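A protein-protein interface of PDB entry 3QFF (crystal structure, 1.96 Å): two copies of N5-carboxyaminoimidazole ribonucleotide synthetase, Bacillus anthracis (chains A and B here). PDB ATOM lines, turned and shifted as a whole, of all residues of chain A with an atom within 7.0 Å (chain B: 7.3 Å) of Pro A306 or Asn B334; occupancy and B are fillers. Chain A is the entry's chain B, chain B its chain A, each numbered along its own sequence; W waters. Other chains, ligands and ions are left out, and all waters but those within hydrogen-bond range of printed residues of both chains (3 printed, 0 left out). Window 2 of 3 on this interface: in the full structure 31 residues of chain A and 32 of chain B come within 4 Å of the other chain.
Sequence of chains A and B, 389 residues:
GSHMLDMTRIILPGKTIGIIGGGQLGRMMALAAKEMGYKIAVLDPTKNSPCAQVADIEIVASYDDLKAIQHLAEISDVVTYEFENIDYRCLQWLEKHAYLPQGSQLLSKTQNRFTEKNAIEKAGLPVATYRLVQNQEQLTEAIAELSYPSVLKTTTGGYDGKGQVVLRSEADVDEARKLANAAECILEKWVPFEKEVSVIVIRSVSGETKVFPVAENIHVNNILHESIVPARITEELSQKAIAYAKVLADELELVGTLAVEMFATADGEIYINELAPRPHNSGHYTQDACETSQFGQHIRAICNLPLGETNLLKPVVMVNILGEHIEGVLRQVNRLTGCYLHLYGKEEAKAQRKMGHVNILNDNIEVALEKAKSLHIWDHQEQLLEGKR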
ATOM      1  N   ILE A  10     -24.038  25.298   5.601  1.00  0.00           N
ATOM      2  CA  ILE A  10     -24.487  26.587   6.133  1.00  0.00           C
ATOM      3  C   ILE A  10     -23.833  27.726   5.368  1.00  0.00           C
ATOM      4  O   ILE A  10     -22.614  27.735   5.175  1.00  0.00           O
ATOM      5  CB  ILE A  10     -24.193  26.713   7.656  1.00  0.00           C
ATOM      6  CG1 ILE A  10     -24.951  25.636   8.442  1.00  0.00           C
ATOM      7  CG2 ILE A  10     -24.556  28.132   8.177  1.00  0.00           C
ATOM      8  CD1 ILE A  10     -24.473  25.421   9.882  1.00  0.00           C
ATOM      9  N   MET A  36     -28.834  40.954   8.257  1.00  0.00           N
ATOM     10  CA  MET A  36     -27.990  39.897   8.808  1.00  0.00           C
ATOM     11  C   MET A  36     -26.517  39.980   8.372  1.00  0.00           C
ATOM     12  O   MET A  36     -25.702  39.200   8.853  1.00  0.00           O
ATOM     13  CB  MET A  36     -28.588  38.510   8.523  1.00  0.00           C
ATOM     14  CG  MET A  36     -29.944  38.295   9.171  1.00  0.00           C
ATOM     15  SD  MET A  36     -30.590  36.608   8.992  1.00  0.00           S
ATOM     16  CE  MET A  36     -29.715  35.808  10.332  1.00  0.00           C
ATOM     17  N   SER A 204     -36.252  24.773   5.906  1.00  0.00           N
ATOM     18  CA  SER A 204     -34.833  25.000   5.694  1.00  0.00           C
ATOM     19  C   SER A 204     -34.165  23.790   5.048  1.00  0.00           C
ATOM     20  O   SER A 204     -34.748  22.702   4.967  1.00  0.00           O
ATOM     21  CB  SER A 204     -34.126  25.358   7.013  1.00  0.00           C
ATOM     22  OG  SER A 204     -33.915  24.208   7.812  1.00  0.00           O
ATOM     23  N   SER A 206     -31.854  21.983   6.263  1.00  0.00           N
ATOM     24  CA  SER A 206     -31.748  20.898   7.239  1.00  0.00           C
ATOM     25  C   SER A 206     -33.107  20.330   7.703  1.00  0.00           C
ATOM     26  O   SER A 206     -33.160  19.520   8.627  1.00  0.00           O
ATOM     27  CB  SER A 206     -30.931  21.365   8.447  1.00  0.00           C
ATOM     28  OG  SER A 206     -31.647  22.359   9.159  1.00  0.00           O
ATOM     29  N   GLU A 208     -35.929  21.910   8.969  1.00  0.00           N
ATOM     30  CA  GLU A 208     -36.731  22.672   9.918  1.00  0.00           C
ATOM     31  C   GLU A 208     -37.904  23.316   9.202  1.00  0.00           C
ATOM     32  O   GLU A 208     -37.731  23.936   8.157  1.00  0.00           O
ATOM     33  CB  GLU A 208     -35.891  23.730  10.649  1.00  0.00           C
ATOM     34  CG  GLU A 208     -36.558  24.205  11.943  1.00  0.00           C
ATOM     35  CD  GLU A 208     -35.897  25.426  12.577  1.00  0.00           C
ATOM     36  OE1 GLU A 208     -34.839  25.887  12.103  1.00  0.00           O
ATOM     37  OE2 GLU A 208     -36.467  25.935  13.564  1.00  0.00           O
ATOM     38  N   LYS A 210     -41.430  25.750   9.478  1.00  0.00           N
ATOM     39  CA  LYS A 210     -42.291  26.711  10.196  1.00  0.00           C
ATOM     40  C   LYS A 210     -43.423  27.178   9.304  1.00  0.00           C
ATOM     41  O   LYS A 210     -43.266  27.292   8.095  1.00  0.00           O
ATOM     42  CB  LYS A 210     -41.498  27.936  10.651  1.00  0.00           C
ATOM     43  CG  LYS A 210     -40.397  27.645  11.641  1.00  0.00           C
ATOM     44  CD  LYS A 210     -40.842  27.817  13.056  1.00  0.00           C
ATOM     45  CE  LYS A 210     -39.619  27.958  13.953  1.00  0.00           C
ATOM     46  NZ  LYS A 210     -39.908  27.339  15.240  1.00  0.00           N
ATOM     47  N   GLY A 296     -37.159  37.306   5.761  1.00  0.00           N
ATOM     48  CA  GLY A 296     -36.092  36.859   6.683  1.00  0.00           C
ATOM     49  C   GLY A 296     -36.086  35.343   6.800  1.00  0.00           C
ATOM     50  O   GLY A 296     -35.028  34.707   6.854  1.00  0.00           O
ATOM     51  N   GLN A 297     -37.279  34.755   6.834  1.00  0.00           N
ATOM     52  CA  GLN A 297     -37.410  33.308   6.880  1.00  0.00           C
ATOM     53  C   GLN A 297     -36.886  32.630   5.615  1.00  0.00           C
ATOM     54  O   GLN A 297     -36.238  31.598   5.702  1.00  0.00           O
ATOM     55  CB  GLN A 297     -38.867  32.916   7.086  1.00  0.00           C
ATOM     56  CG  GLN A 297     -39.390  33.231   8.459  1.00  0.00           C
ATOM     57  CD  GLN A 297     -38.874  32.268   9.517  1.00  0.00           C
ATOM     58  OE1 GLN A 297     -37.665  32.049   9.666  1.00  0.00           O
ATOM     59  NE2 GLN A 297     -39.792  31.694  10.255  1.00  0.00           N
ATOM     60  N   ARG A 300     -33.105  32.700   5.833  1.00  0.00           N
ATOM     61  CA  ARG A 300     -32.646  31.709   6.815  1.00  0.00           C
ATOM     62  C   ARG A 300     -32.815  30.278   6.307  1.00  0.00           C
ATOM     63  O   ARG A 300     -32.028  29.404   6.662  1.00  0.00           O
ATOM     64  CB  ARG A 300     -33.381  31.835   8.152  1.00  0.00           C
ATOM     65  CG  ARG A 300     -33.081  33.102   8.962  1.00  0.00           C
ATOM     66  CD  ARG A 300     -34.211  33.327   9.959  1.00  0.00           C
ATOM     67  NE  ARG A 300     -33.885  34.326  10.975  1.00  0.00           N
ATOM     68  CZ  ARG A 300     -33.815  35.637  10.747  1.00  0.00           C
ATOM     69  NH1 ARG A 300     -34.017  36.117   9.526  1.00  0.00           N
ATOM     70  NH2 ARG A 300     -33.514  36.471  11.739  1.00  0.00           N
ATOM     71  N   ALA A 301     -33.856  30.040   5.505  1.00  0.00           N
ATOM     72  CA  ALA A 301     -34.128  28.694   4.987  1.00  0.00           C
ATOM     73  C   ALA A 301     -33.035  28.220   4.021  1.00  0.00           C
ATOM     74  O   ALA A 301     -32.494  27.136   4.199  1.00  0.00           O
ATOM     75  CB  ALA A 301     -35.500  28.627   4.325  1.00  0.00           C
ATOM     76  N   ASN A 304     -29.597  27.909   5.579  1.00  0.00           N
ATOM     77  CA  ASN A 304     -29.622  26.861   6.603  1.00  0.00           C
ATOM     78  C   ASN A 304     -29.303  27.346   8.023  1.00  0.00           C
ATOM     79  O   ASN A 304     -28.621  26.654   8.802  1.00  0.00           O
ATOM     80  CB  ASN A 304     -28.751  25.661   6.205  1.00  0.00           C
ATOM     81  CG  ASN A 304     -29.136  24.388   6.932  1.00  0.00           C
ATOM     82  OD1 ASN A 304     -30.257  24.250   7.425  1.00  0.00           O
ATOM     83  ND2 ASN A 304     -28.207  23.454   7.010  1.00  0.00           N
ATOM     84  N   LEU A 305     -29.794  28.539   8.349  1.00  0.00           N
ATOM     85  CA  LEU A 305     -29.778  29.036   9.733  1.00  0.00           C
ATOM     86  C   LEU A 305     -31.047  28.578  10.460  1.00  0.00           C
ATOM     87  O   LEU A 305     -32.035  28.199   9.807  1.00  0.00           O
ATOM     88  CB  LEU A 305     -29.685  30.574   9.748  1.00  0.00           C
ATOM     89  CG  LEU A 305     -28.673  31.222   8.804  1.00  0.00           C
ATOM     90  CD1 LEU A 305     -28.853  32.730   8.750  1.00  0.00           C
ATOM     91  CD2 LEU A 305     -27.219  30.848   9.161  1.00  0.00           C
ATOM     92  N   PRO A 306     -31.039  28.600  11.810  1.00  0.00           N
ATOM     93  CA  PRO A 306     -32.302  28.336  12.486  1.00  0.00           C
ATOM     94  C   PRO A 306     -33.363  29.347  12.037  1.00  0.00           C
ATOM     95  O   PRO A 306     -33.062  30.542  11.847  1.00  0.00           O
ATOM     96  CB  PRO A 306     -31.964  28.535  13.973  1.00  0.00           C
ATOM     97  CG  PRO A 306     -30.484  28.381  14.060  1.00  0.00           C
ATOM     98  CD  PRO A 306     -29.950  28.894  12.758  1.00  0.00           C
ATOM     99  N   LEU A 307     -34.579  28.854  11.831  1.00  0.00           N
ATOM    100  CA  LEU A 307     -35.692  29.692  11.436  1.00  0.00           C
ATOM    101  C   LEU A 307     -36.140  30.530  12.636  1.00  0.00           C
ATOM    102  O   LEU A 307     -35.971  30.118  13.796  1.00  0.00           O
ATOM    103  CB  LEU A 307     -36.849  28.835  10.890  1.00  0.00           C
ATOM    104  CG  LEU A 307     -36.535  27.965   9.657  1.00  0.00           C
ATOM    105  CD1 LEU A 307     -37.791  27.249   9.138  1.00  0.00           C
ATOM    106  CD2 LEU A 307     -35.855  28.760   8.519  1.00  0.00           C
ATOM    107  N   GLY A 308     -36.677  31.713  12.344  1.00  0.00           N
ATOM    108  CA  GLY A 308     -37.249  32.564  13.382  1.00  0.00           C
ATOM    109  C   GLY A 308     -38.658  32.116  13.722  1.00  0.00           C
ATOM    110  O   GLY A 308     -39.230  31.267  13.038  1.00  0.00           O
ATOM    111  N   VAL B 329     -20.109  34.038  17.640  1.00  0.00           N
ATOM    112  CA  VAL B 329     -21.446  34.113  17.040  1.00  0.00           C
ATOM    113  C   VAL B 329     -21.544  33.193  15.806  1.00  0.00           C
ATOM    114  O   VAL B 329     -22.462  32.365  15.701  1.00  0.00           O
ATOM    115  CB  VAL B 329     -21.821  35.578  16.663  1.00  0.00           C
ATOM    116  CG1 VAL B 329     -23.127  35.624  15.839  1.00  0.00           C
ATOM    117  CG2 VAL B 329     -21.951  36.452  17.928  1.00  0.00           C
ATOM    118  N   LEU B 330     -20.582  33.325  14.896  1.00  0.00           N
ATOM    119  CA  LEU B 330     -20.613  32.564  13.630  1.00  0.00           C
ATOM    120  C   LEU B 330     -20.507  31.067  13.853  1.00  0.00           C
ATOM    121  O   LEU B 330     -21.138  30.290  13.139  1.00  0.00           O
ATOM    122  CB  LEU B 330     -19.534  33.039  12.656  1.00  0.00           C
ATOM    123  CG  LEU B 330     -19.616  34.481  12.131  1.00  0.00           C
ATOM    124  CD1 LEU B 330     -18.344  34.805  11.381  1.00  0.00           C
ATOM    125  CD2 LEU B 330     -20.833  34.723  11.239  1.00  0.00           C
ATOM    126  N   ARG B 331     -19.733  30.663  14.854  1.00  0.00           N
ATOM    127  CA  ARG B 331     -19.555  29.243  15.140  1.00  0.00           C
ATOM    128  C   ARG B 331     -20.780  28.631  15.823  1.00  0.00           C
ATOM    129  O   ARG B 331     -21.039  27.427  15.695  1.00  0.00           O
ATOM    130  CB  ARG B 331     -18.262  28.997  15.938  1.00  0.00           C
ATOM    131  CG  ARG B 331     -17.006  29.189  15.074  1.00  0.00           C
ATOM    132  CD  ARG B 331     -15.695  28.837  15.781  1.00  0.00           C
ATOM    133  NE  ARG B 331     -15.326  29.832  16.788  1.00  0.00           N
ATOM    134  CZ  ARG B 331     -15.509  29.674  18.097  1.00  0.00           C
ATOM    135  NH1 ARG B 331     -16.049  28.553  18.566  1.00  0.00           N
ATOM    136  NH2 ARG B 331     -15.151  30.633  18.941  1.00  0.00           N
ATOM    137  N   GLN B 332     -21.533  29.471  16.530  1.00  0.00           N
ATOM    138  CA  GLN B 332     -22.706  29.045  17.291  1.00  0.00           C
ATOM    139  C   GLN B 332     -24.008  29.337  16.545  1.00  0.00           C
ATOM    140  O   GLN B 332     -25.085  29.259  17.128  1.00  0.00           O
ATOM    141  CB  GLN B 332     -22.744  29.766  18.647  1.00  0.00           C
ATOM    142  CG  GLN B 332     -21.675  29.336  19.660  1.00  0.00           C
ATOM    143  CD  GLN B 332     -22.036  28.062  20.361  1.00  0.00           C
ATOM    144  OE1 GLN B 332     -22.182  27.019  19.733  1.00  0.00           O
ATOM    145  NE2 GLN B 332     -22.196  28.133  21.673  1.00  0.00           N
ATOM    146  N   VAL B 333     -23.903  29.673  15.261  1.00  0.00           N
ATOM    147  CA  VAL B 333     -25.058  30.119  14.468  1.00  0.00           C
ATOM    148  C   VAL B 333     -26.238  29.135  14.502  1.00  0.00           C
ATOM    149  O   VAL B 333     -27.395  29.548  14.543  1.00  0.00           O
ATOM    150  CB  VAL B 333     -24.644  30.537  13.023  1.00  0.00           C
ATOM    151  CG1 VAL B 333     -24.581  29.343  12.085  1.00  0.00           C
ATOM    152  CG2 VAL B 333     -25.586  31.609  12.479  1.00  0.00           C
ATOM    153  N   ASN B 334     -25.926  27.838  14.545  1.00  0.00           N
ATOM    154  CA  ASN B 334     -26.941  26.789  14.670  1.00  0.00           C
ATOM    155  C   ASN B 334     -27.702  26.797  16.000  1.00  0.00           C
ATOM    156  O   ASN B 334     -28.715  26.122  16.143  1.00  0.00           O
ATOM    157  CB  ASN B 334     -26.308  25.408  14.421  1.00  0.00           C
ATOM    158  CG  ASN B 334     -25.223  25.058  15.442  1.00  0.00           C
ATOM    159  OD1 ASN B 334     -24.407  25.906  15.832  1.00  0.00           O
ATOM    160  ND2 ASN B 334     -25.209  23.798  15.875  1.00  0.00           N
ATOM    161  N   ARG B 335     -27.222  27.562  16.975  1.00  0.00           N
ATOM    162  CA  ARG B 335     -27.864  27.587  18.283  1.00  0.00           C
ATOM    163  C   ARG B 335     -28.687  28.855  18.487  1.00  0.00           C
ATOM    164  O   ARG B 335     -29.163  29.122  19.597  1.00  0.00           O
ATOM    165  CB  ARG B 335     -26.833  27.434  19.406  1.00  0.00           C
ATOM    166  CG  ARG B 335     -25.975  26.184  19.297  1.00  0.00           C
ATOM    167  CD  ARG B 335     -25.895  25.455  20.619  1.00  0.00           C
ATOM    168  NE  ARG B 335     -25.036  26.126  21.596  1.00  0.00           N
ATOM    169  CZ  ARG B 335     -24.674  25.603  22.768  1.00  0.00           C
ATOM    170  NH1 ARG B 335     -25.091  24.391  23.124  1.00  0.00           N
ATOM    171  NH2 ARG B 335     -23.886  26.288  23.589  1.00  0.00           N
ATOM    172  N   LEU B 336     -28.900  29.606  17.406  1.00  0.00           N
ATOM    173  CA  LEU B 336     -29.496  30.936  17.509  1.00  0.00           C
ATOM    174  C   LEU B 336     -31.016  30.979  17.362  1.00  0.00           C
ATOM    175  O   LEU B 336     -31.573  31.986  16.908  1.00  0.00           O
ATOM    176  CB  LEU B 336     -28.819  31.915  16.545  1.00  0.00           C
ATOM    177  CG  LEU B 336     -27.347  32.233  16.831  1.00  0.00           C
ATOM    178  CD1 LEU B 336     -26.790  33.124  15.737  1.00  0.00           C
ATOM    179  CD2 LEU B 336     -27.184  32.900  18.198  1.00  0.00           C
ATOM    180  N   THR B 337     -31.678  29.902  17.784  1.00  0.00           N
ATOM    181  CA  THR B 337     -33.144  29.846  17.857  1.00  0.00           C
ATOM    182  C   THR B 337     -33.713  30.939  18.782  1.00  0.00           C
ATOM    183  O   THR B 337     -33.185  31.178  19.876  1.00  0.00           O
ATOM    184  CB  THR B 337     -33.641  28.438  18.300  1.00  0.00           C
ATOM    185  OG1 THR B 337     -35.081  28.402  18.306  1.00  0.00           O
ATOM    186  CG2 THR B 337     -33.148  28.099  19.680  1.00  0.00           C
ATOM    187  N   GLY B 338     -34.777  31.607  18.333  1.00  0.00           N
ATOM    188  CA  GLY B 338     -35.393  32.697  19.096  1.00  0.00           C
ATOM    189  C   GLY B 338     -34.501  33.931  19.234  1.00  0.00           C
ATOM    190  O   GLY B 338     -34.765  34.803  20.066  1.00  0.00           O
ATOM    191  N   CYS B 339     -33.451  33.992  18.416  1.00  0.00           N
ATOM    192  CA  CYS B 339     -32.488  35.082  18.424  1.00  0.00           C
ATOM    193  C   CYS B 339     -32.523  35.726  17.054  1.00  0.00           C
ATOM    194  O   CYS B 339     -32.651  35.024  16.041  1.00  0.00           O
ATOM    195  CB  CYS B 339     -31.075  34.566  18.706  1.00  0.00           C
ATOM    196  SG  CYS B 339     -30.880  33.716  20.291  1.00  0.00           S
ATOM    197  N   LYS B 371     -30.522  32.307  27.892  1.00  0.00           N
ATOM    198  CA  LYS B 371     -30.132  31.947  26.533  1.00  0.00           C
ATOM    199  C   LYS B 371     -28.778  32.553  26.136  1.00  0.00           C
ATOM    200  O   LYS B 371     -27.915  31.847  25.621  1.00  0.00           O
ATOM    201  CB  LYS B 371     -31.216  32.326  25.513  1.00  0.00           C
ATOM    202  CG  LYS B 371     -30.845  31.967  24.068  1.00  0.00           C
ATOM    203  CD  LYS B 371     -30.870  30.449  23.810  1.00  0.00           C
ATOM    204  CE  LYS B 371     -30.274  30.157  22.433  1.00  0.00           C
ATOM    205  NZ  LYS B 371     -30.133  28.700  22.149  1.00  0.00           N
ATOM    206  N   LEU B 375     -25.053  30.326  25.555  1.00  0.00           N
ATOM    207  CA  LEU B 375     -24.340  30.358  24.286  1.00  0.00           C
ATOM    208  C   LEU B 375     -22.827  30.422  24.463  1.00  0.00           C
ATOM    209  O   LEU B 375     -22.079  30.095  23.541  1.00  0.00           O
ATOM    210  CB  LEU B 375     -24.826  31.534  23.427  1.00  0.00           C
ATOM    211  CG  LEU B 375     -26.261  31.450  22.875  1.00  0.00           C
ATOM    212  CD1 LEU B 375     -26.675  32.757  22.219  1.00  0.00           C
ATOM    213  CD2 LEU B 375     -26.385  30.307  21.875  1.00  0.00           C
HETATM  214  O   HOH W   1     -36.327  31.092  16.249  1.00  0.00           O
HETATM  215  O   HOH W   2     -35.529  27.734  15.075  1.00  0.00           O
HETATM  216  O   HOH W   3     -31.215  35.240  13.465  1.00  0.00           O
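Water W2 lies within hydrogen-bond range of the side-chain carboxylate (OE2) of Glu A208, the backbone carbonyl oxygen (O) of Leu A307 and the side-chain hydroxyl (OG1) of Thr B337. Water W1 lies within hydrogen-bond range of the backbone NH (N) of Gly B338 and the backbone carbonyl oxygen (O) of Leu A307. Water W3 bridges the backbone carbonyl oxygen (O) of Cys B339 (3.0 Å) and the guanidinium group (NH2) of Arg A300 (3.1 Å).
Of chain B, only Val B333, Asn B334 and Leu B336 come within 4 Å of Pro A306. Of chain A, only Pro A306 comes within 4 Å of Asn B334. Of the printed residues of chain A, Val B333 touches Leu A305 and Pro A306. Printed residues of chain B within 4 Å of Leu A305: Val B333 (3.8 Å). Met A36 touches none of the printed residues of chain B. Lys A210 touches none of the printed residues of chain B. The nearest residue of chain B that does not touch Pro A306 is Thr B337 (4.1 Å). The nearest residue of chain A that does not touch Asn B334 is Ile A10 (4.9 Å). The nearest printed residue of chain A that does not touch Leu B336 is Leu A307 (5.7 Å).
Among the printed residues, merely in contact across the chains: Pro A306 with Val B333 (3.2 Å), Pro A306 with Asn B334 (3.5 Å), Leu A305 with Val B333 (3.8 Å) and Pro A306 with Leu B336 (3.9 Å).
The backbone carbonyl oxygen (O) of Arg A300 is in hydrogen-bond range of the backbone NH (N) of Leu A305 (2.9 Å).
Of the 15 printed residues of chain A, 2 touch a printed residue of chain B. Hydrophobic or aromatic side chains of chain A that line the printed part of chain B: Leu A305 and Pro A306. Among the printed residues, no Asp or Glu carboxylate lies within 4 Å of a Lys or Arg side-chain nitrogen of the other chain.
No position is printed for both chains. Of the 4 pairs that touch across the chains among the printed residues, none has its exchanged pair printed and touching as well.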
